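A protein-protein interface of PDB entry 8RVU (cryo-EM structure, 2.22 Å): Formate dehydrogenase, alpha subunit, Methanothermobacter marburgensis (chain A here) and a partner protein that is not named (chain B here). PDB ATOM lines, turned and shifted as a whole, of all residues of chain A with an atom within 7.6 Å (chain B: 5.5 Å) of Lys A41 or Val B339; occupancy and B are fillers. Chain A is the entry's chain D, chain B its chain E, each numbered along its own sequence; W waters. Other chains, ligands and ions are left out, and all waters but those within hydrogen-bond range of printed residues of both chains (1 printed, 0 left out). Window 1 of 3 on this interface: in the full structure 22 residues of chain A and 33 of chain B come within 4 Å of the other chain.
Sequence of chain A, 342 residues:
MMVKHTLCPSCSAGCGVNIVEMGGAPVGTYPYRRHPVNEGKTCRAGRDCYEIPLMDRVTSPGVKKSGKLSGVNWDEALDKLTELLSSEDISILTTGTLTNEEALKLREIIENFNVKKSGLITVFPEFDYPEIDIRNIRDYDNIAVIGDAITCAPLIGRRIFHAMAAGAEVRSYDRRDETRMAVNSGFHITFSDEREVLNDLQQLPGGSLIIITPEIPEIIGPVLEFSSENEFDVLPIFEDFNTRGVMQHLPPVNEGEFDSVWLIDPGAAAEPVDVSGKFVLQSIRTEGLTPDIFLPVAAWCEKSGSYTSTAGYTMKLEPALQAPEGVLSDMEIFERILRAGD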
ATOM      1  N   CYS A  15      28.156   7.470 -23.087  1.00  0.00           N
ATOM      2  CA  CYS A  15      26.905   7.484 -22.341  1.00  0.00           C
ATOM      3  C   CYS A  15      26.693   8.830 -21.660  1.00  0.00           C
ATOM      4  O   CYS A  15      27.618   9.409 -21.086  1.00  0.00           O
ATOM      5  CB  CYS A  15      26.900   6.368 -21.299  1.00  0.00           C
ATOM      6  SG  CYS A  15      27.016   4.712 -22.002  1.00  0.00           S
ATOM      7  N   GLY A  16      25.459   9.325 -21.725  1.00  0.00           N
ATOM      8  CA  GLY A  16      25.099  10.564 -21.058  1.00  0.00           C
ATOM      9  C   GLY A  16      24.466  10.302 -19.701  1.00  0.00           C
ATOM     10  O   GLY A  16      23.743   9.326 -19.514  1.00  0.00           O
ATOM     11  N   VAL A  17      24.751  11.195 -18.752  1.00  0.00           N
ATOM     12  CA  VAL A  17      24.208  11.122 -17.404  1.00  0.00           C
ATOM     13  C   VAL A  17      23.750  12.517 -17.005  1.00  0.00           C
ATOM     14  O   VAL A  17      24.036  13.505 -17.685  1.00  0.00           O
ATOM     15  CB  VAL A  17      25.237  10.581 -16.386  1.00  0.00           C
ATOM     16  CG1 VAL A  17      25.720   9.206 -16.802  1.00  0.00           C
ATOM     17  CG2 VAL A  17      26.410  11.536 -16.243  1.00  0.00           C
ATOM     18  N   TYR A  30      21.146  11.271 -12.150  1.00  0.00           N
ATOM     19  CA  TYR A  30      19.807  11.120 -12.692  1.00  0.00           C
ATOM     20  C   TYR A  30      19.882  10.579 -14.114  1.00  0.00           C
ATOM     21  O   TYR A  30      20.850  10.850 -14.840  1.00  0.00           O
ATOM     22  CB  TYR A  30      19.054  12.462 -12.681  1.00  0.00           C
ATOM     23  CG  TYR A  30      17.548  12.334 -12.618  1.00  0.00           C
ATOM     24  CD1 TYR A  30      16.918  11.911 -11.457  1.00  0.00           C
ATOM     25  CD2 TYR A  30      16.756  12.642 -13.717  1.00  0.00           C
ATOM     26  CE1 TYR A  30      15.543  11.795 -11.389  1.00  0.00           C
ATOM     27  CE2 TYR A  30      15.378  12.528 -13.659  1.00  0.00           C
ATOM     28  CZ  TYR A  30      14.778  12.105 -12.492  1.00  0.00           C
ATOM     29  OH  TYR A  30      13.408  11.989 -12.426  1.00  0.00           O
ATOM     30  N   PRO A  31      18.881   9.801 -14.538  1.00  0.00           N
ATOM     31  CA  PRO A  31      18.928   9.212 -15.885  1.00  0.00           C
ATOM     32  C   PRO A  31      18.824  10.276 -16.970  1.00  0.00           C
ATOM     33  O   PRO A  31      17.968  11.160 -16.914  1.00  0.00           O
ATOM     34  CB  PRO A  31      17.717   8.271 -15.908  1.00  0.00           C
ATOM     35  CG  PRO A  31      17.411   7.998 -14.487  1.00  0.00           C
ATOM     36  CD  PRO A  31      17.759   9.254 -13.753  1.00  0.00           C
ATOM     37  N   TYR A  32      19.703  10.172 -17.963  1.00  0.00           N
ATOM     38  CA  TYR A  32      19.677  11.049 -19.131  1.00  0.00           C
ATOM     39  C   TYR A  32      19.005  10.305 -20.286  1.00  0.00           C
ATOM     40  O   TYR A  32      19.639   9.832 -21.230  1.00  0.00           O
ATOM     41  CB  TYR A  32      21.099  11.493 -19.474  1.00  0.00           C
ATOM     42  CG  TYR A  32      21.226  12.575 -20.529  1.00  0.00           C
ATOM     43  CD1 TYR A  32      20.125  13.033 -21.243  1.00  0.00           C
ATOM     44  CD2 TYR A  32      22.464  13.139 -20.810  1.00  0.00           C
ATOM     45  CE1 TYR A  32      20.255  14.019 -22.203  1.00  0.00           C
ATOM     46  CE2 TYR A  32      22.602  14.123 -21.767  1.00  0.00           C
ATOM     47  CZ  TYR A  32      21.496  14.560 -22.461  1.00  0.00           C
ATOM     48  OH  TYR A  32      21.630  15.542 -23.414  1.00  0.00           O
ATOM     49  N   ARG A  33      17.675  10.216 -20.191  1.00  0.00           N
ATOM     50  CA  ARG A  33      16.907   9.372 -21.101  1.00  0.00           C
ATOM     51  C   ARG A  33      17.002   9.829 -22.550  1.00  0.00           C
ATOM     52  O   ARG A  33      16.869   9.002 -23.458  1.00  0.00           O
ATOM     53  CB  ARG A  33      15.439   9.345 -20.671  1.00  0.00           C
ATOM     54  CG  ARG A  33      15.134   8.344 -19.569  1.00  0.00           C
ATOM     55  CD  ARG A  33      13.648   8.299 -19.246  1.00  0.00           C
ATOM     56  NE  ARG A  33      13.360   7.402 -18.134  1.00  0.00           N
ATOM     57  CZ  ARG A  33      13.419   7.745 -16.854  1.00  0.00           C
ATOM     58  NH1 ARG A  33      13.749   8.970 -16.478  1.00  0.00           N
ATOM     59  NH2 ARG A  33      13.142   6.835 -15.925  1.00  0.00           N
ATOM     60  N   HIS A  35      19.586  10.966 -24.210  1.00  0.00           N
ATOM     61  CA  HIS A  35      20.851  10.732 -24.889  1.00  0.00           C
ATOM     62  C   HIS A  35      20.738   9.511 -25.803  1.00  0.00           C
ATOM     63  O   HIS A  35      20.179   8.486 -25.403  1.00  0.00           O
ATOM     64  CB  HIS A  35      21.973  10.522 -23.875  1.00  0.00           C
ATOM     65  CG  HIS A  35      23.336  10.795 -24.427  1.00  0.00           C
ATOM     66  ND1 HIS A  35      24.037   9.873 -25.174  1.00  0.00           N
ATOM     67  CD2 HIS A  35      24.130  11.888 -24.340  1.00  0.00           C
ATOM     68  CE1 HIS A  35      25.201  10.389 -25.527  1.00  0.00           C
ATOM     69  NE2 HIS A  35      25.284  11.609 -25.031  1.00  0.00           N
ATOM     70  N   VAL A  37      23.174   7.480 -27.144  1.00  0.00           N
ATOM     71  CA  VAL A  37      24.109   6.372 -26.974  1.00  0.00           C
ATOM     72  C   VAL A  37      23.532   5.321 -26.033  1.00  0.00           C
ATOM     73  O   VAL A  37      23.625   4.117 -26.299  1.00  0.00           O
ATOM     74  CB  VAL A  37      25.469   6.893 -26.474  1.00  0.00           C
ATOM     75  CG1 VAL A  37      26.280   5.766 -25.847  1.00  0.00           C
ATOM     76  CG2 VAL A  37      26.240   7.534 -27.615  1.00  0.00           C
ATOM     77  N   ASN A  38      22.927   5.752 -24.925  1.00  0.00           N
ATOM     78  CA  ASN A  38      22.471   4.831 -23.893  1.00  0.00           C
ATOM     79  C   ASN A  38      21.023   5.024 -23.470  1.00  0.00           C
ATOM     80  O   ASN A  38      20.493   4.157 -22.767  1.00  0.00           O
ATOM     81  CB  ASN A  38      23.365   4.945 -22.651  1.00  0.00           C
ATOM     82  CG  ASN A  38      23.371   6.343 -22.057  1.00  0.00           C
ATOM     83  OD1 ASN A  38      23.405   7.337 -22.780  1.00  0.00           O
ATOM     84  ND2 ASN A  38      23.341   6.422 -20.733  1.00  0.00           N
ATOM     85  N   GLU A  39      20.366   6.114 -23.868  1.00  0.00           N
ATOM     86  CA  GLU A  39      18.952   6.335 -23.563  1.00  0.00           C
ATOM     87  C   GLU A  39      18.682   6.249 -22.061  1.00  0.00           C
ATOM     88  O   GLU A  39      17.682   5.676 -21.625  1.00  0.00           O
ATOM     89  CB  GLU A  39      18.066   5.349 -24.325  1.00  0.00           C
ATOM     90  CG  GLU A  39      18.644   4.893 -25.656  1.00  0.00           C
ATOM     91  CD  GLU A  39      17.609   4.241 -26.553  1.00  0.00           C
ATOM     92  OE1 GLU A  39      16.411   4.568 -26.421  1.00  0.00           O
ATOM     93  OE2 GLU A  39      17.995   3.400 -27.391  1.00  0.00           O
ATOM     94  N   GLY A  40      19.575   6.825 -21.263  1.00  0.00           N
ATOM     95  CA  GLY A  40      19.384   6.869 -19.828  1.00  0.00           C
ATOM     96  C   GLY A  40      19.820   5.633 -19.078  1.00  0.00           C
ATOM     97  O   GLY A  40      19.639   5.575 -17.856  1.00  0.00           O
ATOM     98  N   LYS A  41      20.387   4.644 -19.761  1.00  0.00           N
ATOM     99  CA  LYS A  41      20.869   3.425 -19.126  1.00  0.00           C
ATOM    100  C   LYS A  41      22.364   3.550 -18.869  1.00  0.00           C
ATOM    101  O   LYS A  41      23.118   3.960 -19.754  1.00  0.00           O
ATOM    102  CB  LYS A  41      20.581   2.203 -20.000  1.00  0.00           C
ATOM    103  CG  LYS A  41      19.124   2.047 -20.401  1.00  0.00           C
ATOM    104  CD  LYS A  41      18.974   1.097 -21.578  1.00  0.00           C
ATOM    105  CE  LYS A  41      17.515   0.883 -21.944  1.00  0.00           C
ATOM    106  NZ  LYS A  41      16.806   0.042 -20.940  1.00  0.00           N
ATOM    107  N   THR A  42      22.786   3.202 -17.659  1.00  0.00           N
ATOM    108  CA  THR A  42      24.185   3.297 -17.275  1.00  0.00           C
ATOM    109  C   THR A  42      24.591   2.069 -16.478  1.00  0.00           C
ATOM    110  O   THR A  42      23.764   1.436 -15.816  1.00  0.00           O
ATOM    111  CB  THR A  42      24.462   4.555 -16.438  1.00  0.00           C
ATOM    112  OG1 THR A  42      23.454   4.695 -15.431  1.00  0.00           O
ATOM    113  CG2 THR A  42      24.477   5.792 -17.315  1.00  0.00           C
ATOM    114  N   CYS A  43      25.876   1.738 -16.553  1.00  0.00           N
ATOM    115  CA  CYS A  43      26.461   0.757 -15.656  1.00  0.00           C
ATOM    116  C   CYS A  43      26.747   1.419 -14.309  1.00  0.00           C
ATOM    117  O   CYS A  43      26.417   2.585 -14.078  1.00  0.00           O
ATOM    118  CB  CYS A  43      27.725   0.161 -16.268  1.00  0.00           C
ATOM    119  SG  CYS A  43      29.148   1.272 -16.266  1.00  0.00           S
ATOM    120  N   GLY A  46      28.845   4.677 -14.378  1.00  0.00           N
ATOM    121  CA  GLY A  46      28.111   5.851 -14.821  1.00  0.00           C
ATOM    122  C   GLY A  46      27.310   6.489 -13.704  1.00  0.00           C
ATOM    123  O   GLY A  46      27.183   7.714 -13.639  1.00  0.00           O
ATOM    124  N   ARG A  47      26.754   5.670 -12.811  1.00  0.00           N
ATOM    125  CA  ARG A  47      26.001   6.195 -11.681  1.00  0.00           C
ATOM    126  C   ARG A  47      26.898   6.607 -10.521  1.00  0.00           C
ATOM    127  O   ARG A  47      26.438   7.325  -9.627  1.00  0.00           O
ATOM    128  CB  ARG A  47      24.977   5.157 -11.213  1.00  0.00           C
ATOM    129  CG  ARG A  47      23.599   5.350 -11.827  1.00  0.00           C
ATOM    130  CD  ARG A  47      22.734   4.107 -11.707  1.00  0.00           C
ATOM    131  NE  ARG A  47      23.189   3.033 -12.582  1.00  0.00           N
ATOM    132  CZ  ARG A  47      23.680   1.869 -12.173  1.00  0.00           C
ATOM    133  NH1 ARG A  47      23.812   1.580 -10.888  1.00  0.00           N
ATOM    134  NH2 ARG A  47      24.046   0.968 -13.078  1.00  0.00           N
ATOM    135  N   LEU A 155      27.535  -0.610 -22.452  1.00  0.00           N
ATOM    136  CA  LEU A 155      26.500  -0.083 -23.331  1.00  0.00           C
ATOM    137  C   LEU A 155      26.810  -0.301 -24.807  1.00  0.00           C
ATOM    138  O   LEU A 155      25.941  -0.045 -25.647  1.00  0.00           O
ATOM    139  CB  LEU A 155      26.286   1.408 -23.049  1.00  0.00           C
ATOM    140  CG  LEU A 155      25.201   1.746 -22.018  1.00  0.00           C
ATOM    141  CD1 LEU A 155      23.831   1.236 -22.444  1.00  0.00           C
ATOM    142  CD2 LEU A 155      25.566   1.194 -20.647  1.00  0.00           C
ATOM    143  N   ARG A 158      25.561  -3.953 -25.031  1.00  0.00           N
ATOM    144  CA  ARG A 158      24.115  -3.914 -25.222  1.00  0.00           C
ATOM    145  C   ARG A 158      23.763  -3.927 -26.707  1.00  0.00           C
ATOM    146  O   ARG A 158      22.853  -4.647 -27.137  1.00  0.00           O
ATOM    147  CB  ARG A 158      23.537  -2.676 -24.534  1.00  0.00           C
ATOM    148  CG  ARG A 158      22.239  -2.149 -25.124  1.00  0.00           C
ATOM    149  CD  ARG A 158      21.704  -0.993 -24.296  1.00  0.00           C
ATOM    150  NE  ARG A 158      20.278  -0.773 -24.505  1.00  0.00           N
ATOM    151  CZ  ARG A 158      19.757   0.201 -25.240  1.00  0.00           C
ATOM    152  NH1 ARG A 158      20.519   1.068 -25.888  1.00  0.00           N
ATOM    153  NH2 ARG A 158      18.435   0.308 -25.329  1.00  0.00           N
ATOM    154  N   HIS A 162      21.785  -6.601 -29.054  1.00  0.00           N
ATOM    155  CA  HIS A 162      20.772  -6.242 -30.043  1.00  0.00           C
ATOM    156  C   HIS A 162      21.081  -6.878 -31.393  1.00  0.00           C
ATOM    157  O   HIS A 162      20.180  -7.378 -32.077  1.00  0.00           O
ATOM    158  CB  HIS A 162      20.688  -4.722 -30.185  1.00  0.00           C
ATOM    159  CG  HIS A 162      19.934  -4.047 -29.081  1.00  0.00           C
ATOM    160  ND1 HIS A 162      19.758  -2.681 -29.033  1.00  0.00           N
ATOM    161  CD2 HIS A 162      19.312  -4.546 -27.988  1.00  0.00           C
ATOM    162  CE1 HIS A 162      19.059  -2.369 -27.957  1.00  0.00           C
ATOM    163  NE2 HIS A 162      18.776  -3.482 -27.305  1.00  0.00           N
ATOM    164  N   ALA B 285      21.361  -0.962 -11.613  1.00  0.00           N
ATOM    165  CA  ALA B 285      20.603   0.189 -12.090  1.00  0.00           C
ATOM    166  C   ALA B 285      19.136   0.070 -11.702  1.00  0.00           C
ATOM    167  O   ALA B 285      18.498   1.064 -11.344  1.00  0.00           O
ATOM    168  CB  ALA B 285      20.747   0.329 -13.604  1.00  0.00           C
ATOM    169  N   CYS B 286      18.586  -1.143 -11.771  1.00  0.00           N
ATOM    170  CA  CYS B 286      17.187  -1.347 -11.413  1.00  0.00           C
ATOM    171  C   CYS B 286      16.939  -0.998  -9.951  1.00  0.00           C
ATOM    172  O   CYS B 286      15.977  -0.295  -9.622  1.00  0.00           O
ATOM    173  CB  CYS B 286      16.785  -2.794 -11.700  1.00  0.00           C
ATOM    174  SG  CYS B 286      18.017  -4.024 -11.205  1.00  0.00           S
ATOM    175  N   ALA B 289      17.205   2.777  -9.397  1.00  0.00           N
ATOM    176  CA  ALA B 289      16.052   3.492  -9.926  1.00  0.00           C
ATOM    177  C   ALA B 289      14.777   3.207  -9.145  1.00  0.00           C
ATOM    178  O   ALA B 289      13.866   4.039  -9.154  1.00  0.00           O
ATOM    179  CB  ALA B 289      15.846   3.132 -11.396  1.00  0.00           C
ATOM    180  N   GLY B 334       7.929   1.145 -13.494  1.00  0.00           N
ATOM    181  CA  GLY B 334       8.695   0.844 -14.688  1.00  0.00           C
ATOM    182  C   GLY B 334      10.078   1.449 -14.757  1.00  0.00           C
ATOM    183  O   GLY B 334      10.729   1.336 -15.798  1.00  0.00           O
ATOM    184  N   GLN B 335      10.553   2.092 -13.687  1.00  0.00           N
ATOM    185  CA  GLN B 335      11.875   2.710 -13.726  1.00  0.00           C
ATOM    186  C   GLN B 335      12.975   1.661 -13.850  1.00  0.00           C
ATOM    187  O   GLN B 335      13.959   1.864 -14.575  1.00  0.00           O
ATOM    188  CB  GLN B 335      12.091   3.562 -12.475  1.00  0.00           C
ATOM    189  CG  GLN B 335      11.063   4.664 -12.287  1.00  0.00           C
ATOM    190  CD  GLN B 335      11.200   5.769 -13.313  1.00  0.00           C
ATOM    191  OE1 GLN B 335      12.309   6.175 -13.659  1.00  0.00           O
ATOM    192  NE2 GLN B 335      10.071   6.262 -13.806  1.00  0.00           N
ATOM    193  N   CYS B 336      12.828   0.538 -13.143  1.00  0.00           N
ATOM    194  CA  CYS B 336      13.841  -0.510 -13.196  1.00  0.00           C
ATOM    195  C   CYS B 336      14.030  -1.017 -14.618  1.00  0.00           C
ATOM    196  O   CYS B 336      15.163  -1.202 -15.077  1.00  0.00           O
ATOM    197  CB  CYS B 336      13.451  -1.659 -12.269  1.00  0.00           C
ATOM    198  SG  CYS B 336      11.753  -2.241 -12.495  1.00  0.00           S
ATOM    199  N   GLU B 337      12.927  -1.250 -15.331  1.00  0.00           N
ATOM    200  CA  GLU B 337      13.018  -1.661 -16.725  1.00  0.00           C
ATOM    201  C   GLU B 337      13.541  -0.535 -17.605  1.00  0.00           C
ATOM    202  O   GLU B 337      14.251  -0.793 -18.584  1.00  0.00           O
ATOM    203  CB  GLU B 337      11.649  -2.124 -17.221  1.00  0.00           C
ATOM    204  CG  GLU B 337      11.715  -3.284 -18.183  1.00  0.00           C
ATOM    205  CD  GLU B 337      10.373  -3.601 -18.810  1.00  0.00           C
ATOM    206  OE1 GLU B 337       9.446  -3.995 -18.071  1.00  0.00           O
ATOM    207  OE2 GLU B 337      10.248  -3.461 -20.044  1.00  0.00           O
ATOM    208  N   ASP B 338      13.202   0.712 -17.276  1.00  0.00           N
ATOM    209  CA  ASP B 338      13.667   1.843 -18.071  1.00  0.00           C
ATOM    210  C   ASP B 338      15.186   1.947 -18.052  1.00  0.00           C
ATOM    211  O   ASP B 338      15.808   2.216 -19.085  1.00  0.00           O
ATOM    212  CB  ASP B 338      13.045   3.138 -17.549  1.00  0.00           C
ATOM    213  CG  ASP B 338      11.622   3.339 -18.025  1.00  0.00           C
ATOM    214  OD1 ASP B 338      11.232   2.720 -19.037  1.00  0.00           O
ATOM    215  OD2 ASP B 338      10.891   4.120 -17.382  1.00  0.00           O
ATOM    216  N   VAL B 339      15.803   1.741 -16.884  1.00  0.00           N
ATOM    217  CA  VAL B 339      17.232   2.007 -16.734  1.00  0.00           C
ATOM    218  C   VAL B 339      18.102   0.782 -16.980  1.00  0.00           C
ATOM    219  O   VAL B 339      19.335   0.896 -16.925  1.00  0.00           O
ATOM    220  CB  VAL B 339      17.547   2.568 -15.331  1.00  0.00           C
ATOM    221  CG1 VAL B 339      16.755   3.840 -15.079  1.00  0.00           C
ATOM    222  CG2 VAL B 339      17.266   1.528 -14.254  1.00  0.00           C
ATOM    223  N   CYS B 340      17.517  -0.375 -17.255  1.00  0.00           N
ATOM    224  CA  CYS B 340      18.309  -1.598 -17.352  1.00  0.00           C
ATOM    225  C   CYS B 340      19.211  -1.551 -18.579  1.00  0.00           C
ATOM    226  O   CYS B 340      18.703  -1.425 -19.701  1.00  0.00           O
ATOM    227  CB  CYS B 340      17.401  -2.820 -17.416  1.00  0.00           C
ATOM    228  SG  CYS B 340      18.300  -4.386 -17.494  1.00  0.00           S
ATOM    229  N   PRO B 341      20.537  -1.657 -18.431  1.00  0.00           N
ATOM    230  CA  PRO B 341      21.410  -1.645 -19.617  1.00  0.00           C
ATOM    231  C   PRO B 341      21.272  -2.876 -20.499  1.00  0.00           C
ATOM    232  O   PRO B 341      21.635  -2.807 -21.678  1.00  0.00           O
ATOM    233  CB  PRO B 341      22.827  -1.551 -19.026  1.00  0.00           C
ATOM    234  CG  PRO B 341      22.668  -1.370 -17.555  1.00  0.00           C
ATOM    235  CD  PRO B 341      21.303  -1.822 -17.183  1.00  0.00           C
ATOM    236  N   ASP B 343      18.357  -4.552 -21.126  1.00  0.00           N
ATOM    237  CA  ASP B 343      17.019  -4.653 -21.705  1.00  0.00           C
ATOM    238  C   ASP B 343      16.300  -5.917 -21.223  1.00  0.00           C
ATOM    239  O   ASP B 343      15.852  -6.752 -22.010  1.00  0.00           O
ATOM    240  CB  ASP B 343      17.088  -4.614 -23.237  1.00  0.00           C
ATOM    241  CG  ASP B 343      17.565  -3.279 -23.765  1.00  0.00           C
ATOM    242  OD1 ASP B 343      16.815  -2.288 -23.656  1.00  0.00           O
ATOM    243  OD2 ASP B 343      18.694  -3.222 -24.294  1.00  0.00           O
HETATM  244  O   HOH W   1      13.155   9.200 -13.456  1.00  0.00           O
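Glu B337 touches Lys A41 (O to NZ, 3.6 Å).
CB of Lys A41 touches O of Val B339, 3.6 Å away.
CB of Lys A41 touches CA of Pro B341 (3.95 Å).
Ala B285 touches Thr A42.
Thr A42 touches Pro B341.
Ala B285 touches Arg A47 (CB to NH2, 3.4 Å).
O of Pro B341 touches CD of Arg A158, at 3.2 Å.
Of the 12 printed residues of chain B, 8 touch a printed residue of chain A.
Along chain B the printed residues that touch a printed residue of chain A span positions 285 to 343.
Among the printed residues, 14 pairs touch across the chains.
Among the printed residues, Asp or Glu carboxylates within 4 Å of a Lys or Arg side-chain nitrogen of the other chain: Arg A33 with Asp B338, Lys A41 with Asp B343 and Arg A158 with Asp B343.
OD2 of Asp B343 lies within salt-bridge range of NE of Arg A158, at 2.9 Å.
NH2 of Arg A33 is in hydrogen-bond range of OE1 of Gln B335, at 2.5 Å.
The side-chain carboxylate (OD2) of Asp B338 lies within salt-bridge range of the guanidinium group (NH2) of Arg A33 (3.8 Å).
The side-chain amino group (NZ) of Lys A41 lies within hydrogen-bond range of the backbone carbonyl oxygen (O) of Cys B340.
The side-chain carboxylate of Asp B343 lies within hydrogen-bond range of a ring nitrogen (NE2) of His A162 (3.0 Å).
The side-chain amino group (NZ) of Lys A41 lies within hydrogen-bond range of the backbone carbonyl oxygen (O) of Asp B338, 3.0 Å away.
OD1 of Asp B343 is in salt-bridge range of NZ of Lys A41, 3.6 Å away.
The backbone carbonyl oxygen of Thr A42 sits at hydrogen-bond distance from the guanidinium group of Arg A47 (2.8 Å).
O of Cys A43 sits close to NH2 of Arg A47.
The backbone NH of Asp B343 lies close to the side-chain sulfur of Cys B340.
The side-chain carboxylate (OE2) of Glu A39 lies within salt-bridge range of the guanidinium group (NH2) of Arg A158, at 3.7 Å.
The backbone carbonyl oxygen of Lys A41 sits at hydrogen-bond distance from the side-chain amide nitrogen of Asn A38 (2.7 Å).
Of the printed residues of chain A, Val B339 touches Lys A41 (3.6 Å).
Printed residues of chain B within 4 Å of Thr A42: Ala B285 and Pro B341.
Printed residues of chain A within 4 Å of Asp B343: Lys A41, Arg A158 and His A162.
Of the printed residues of chain A, Asp B338 touches Arg A33 and Lys A41.
Of the printed residues of chain B, Arg A158 touches Pro B341 (3.2 Å) and Asp B343 (2.9 Å).
The nearest printed residue of chain B that does not touch Lys A41 is Cys B336 (6.2 Å).
Water W1 lies within hydrogen-bond range of OH of Tyr A30 (3.0 Å), NH1 of Arg A33 (3.1 Å) and OE1 of Gln B335 (3.1 Å).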
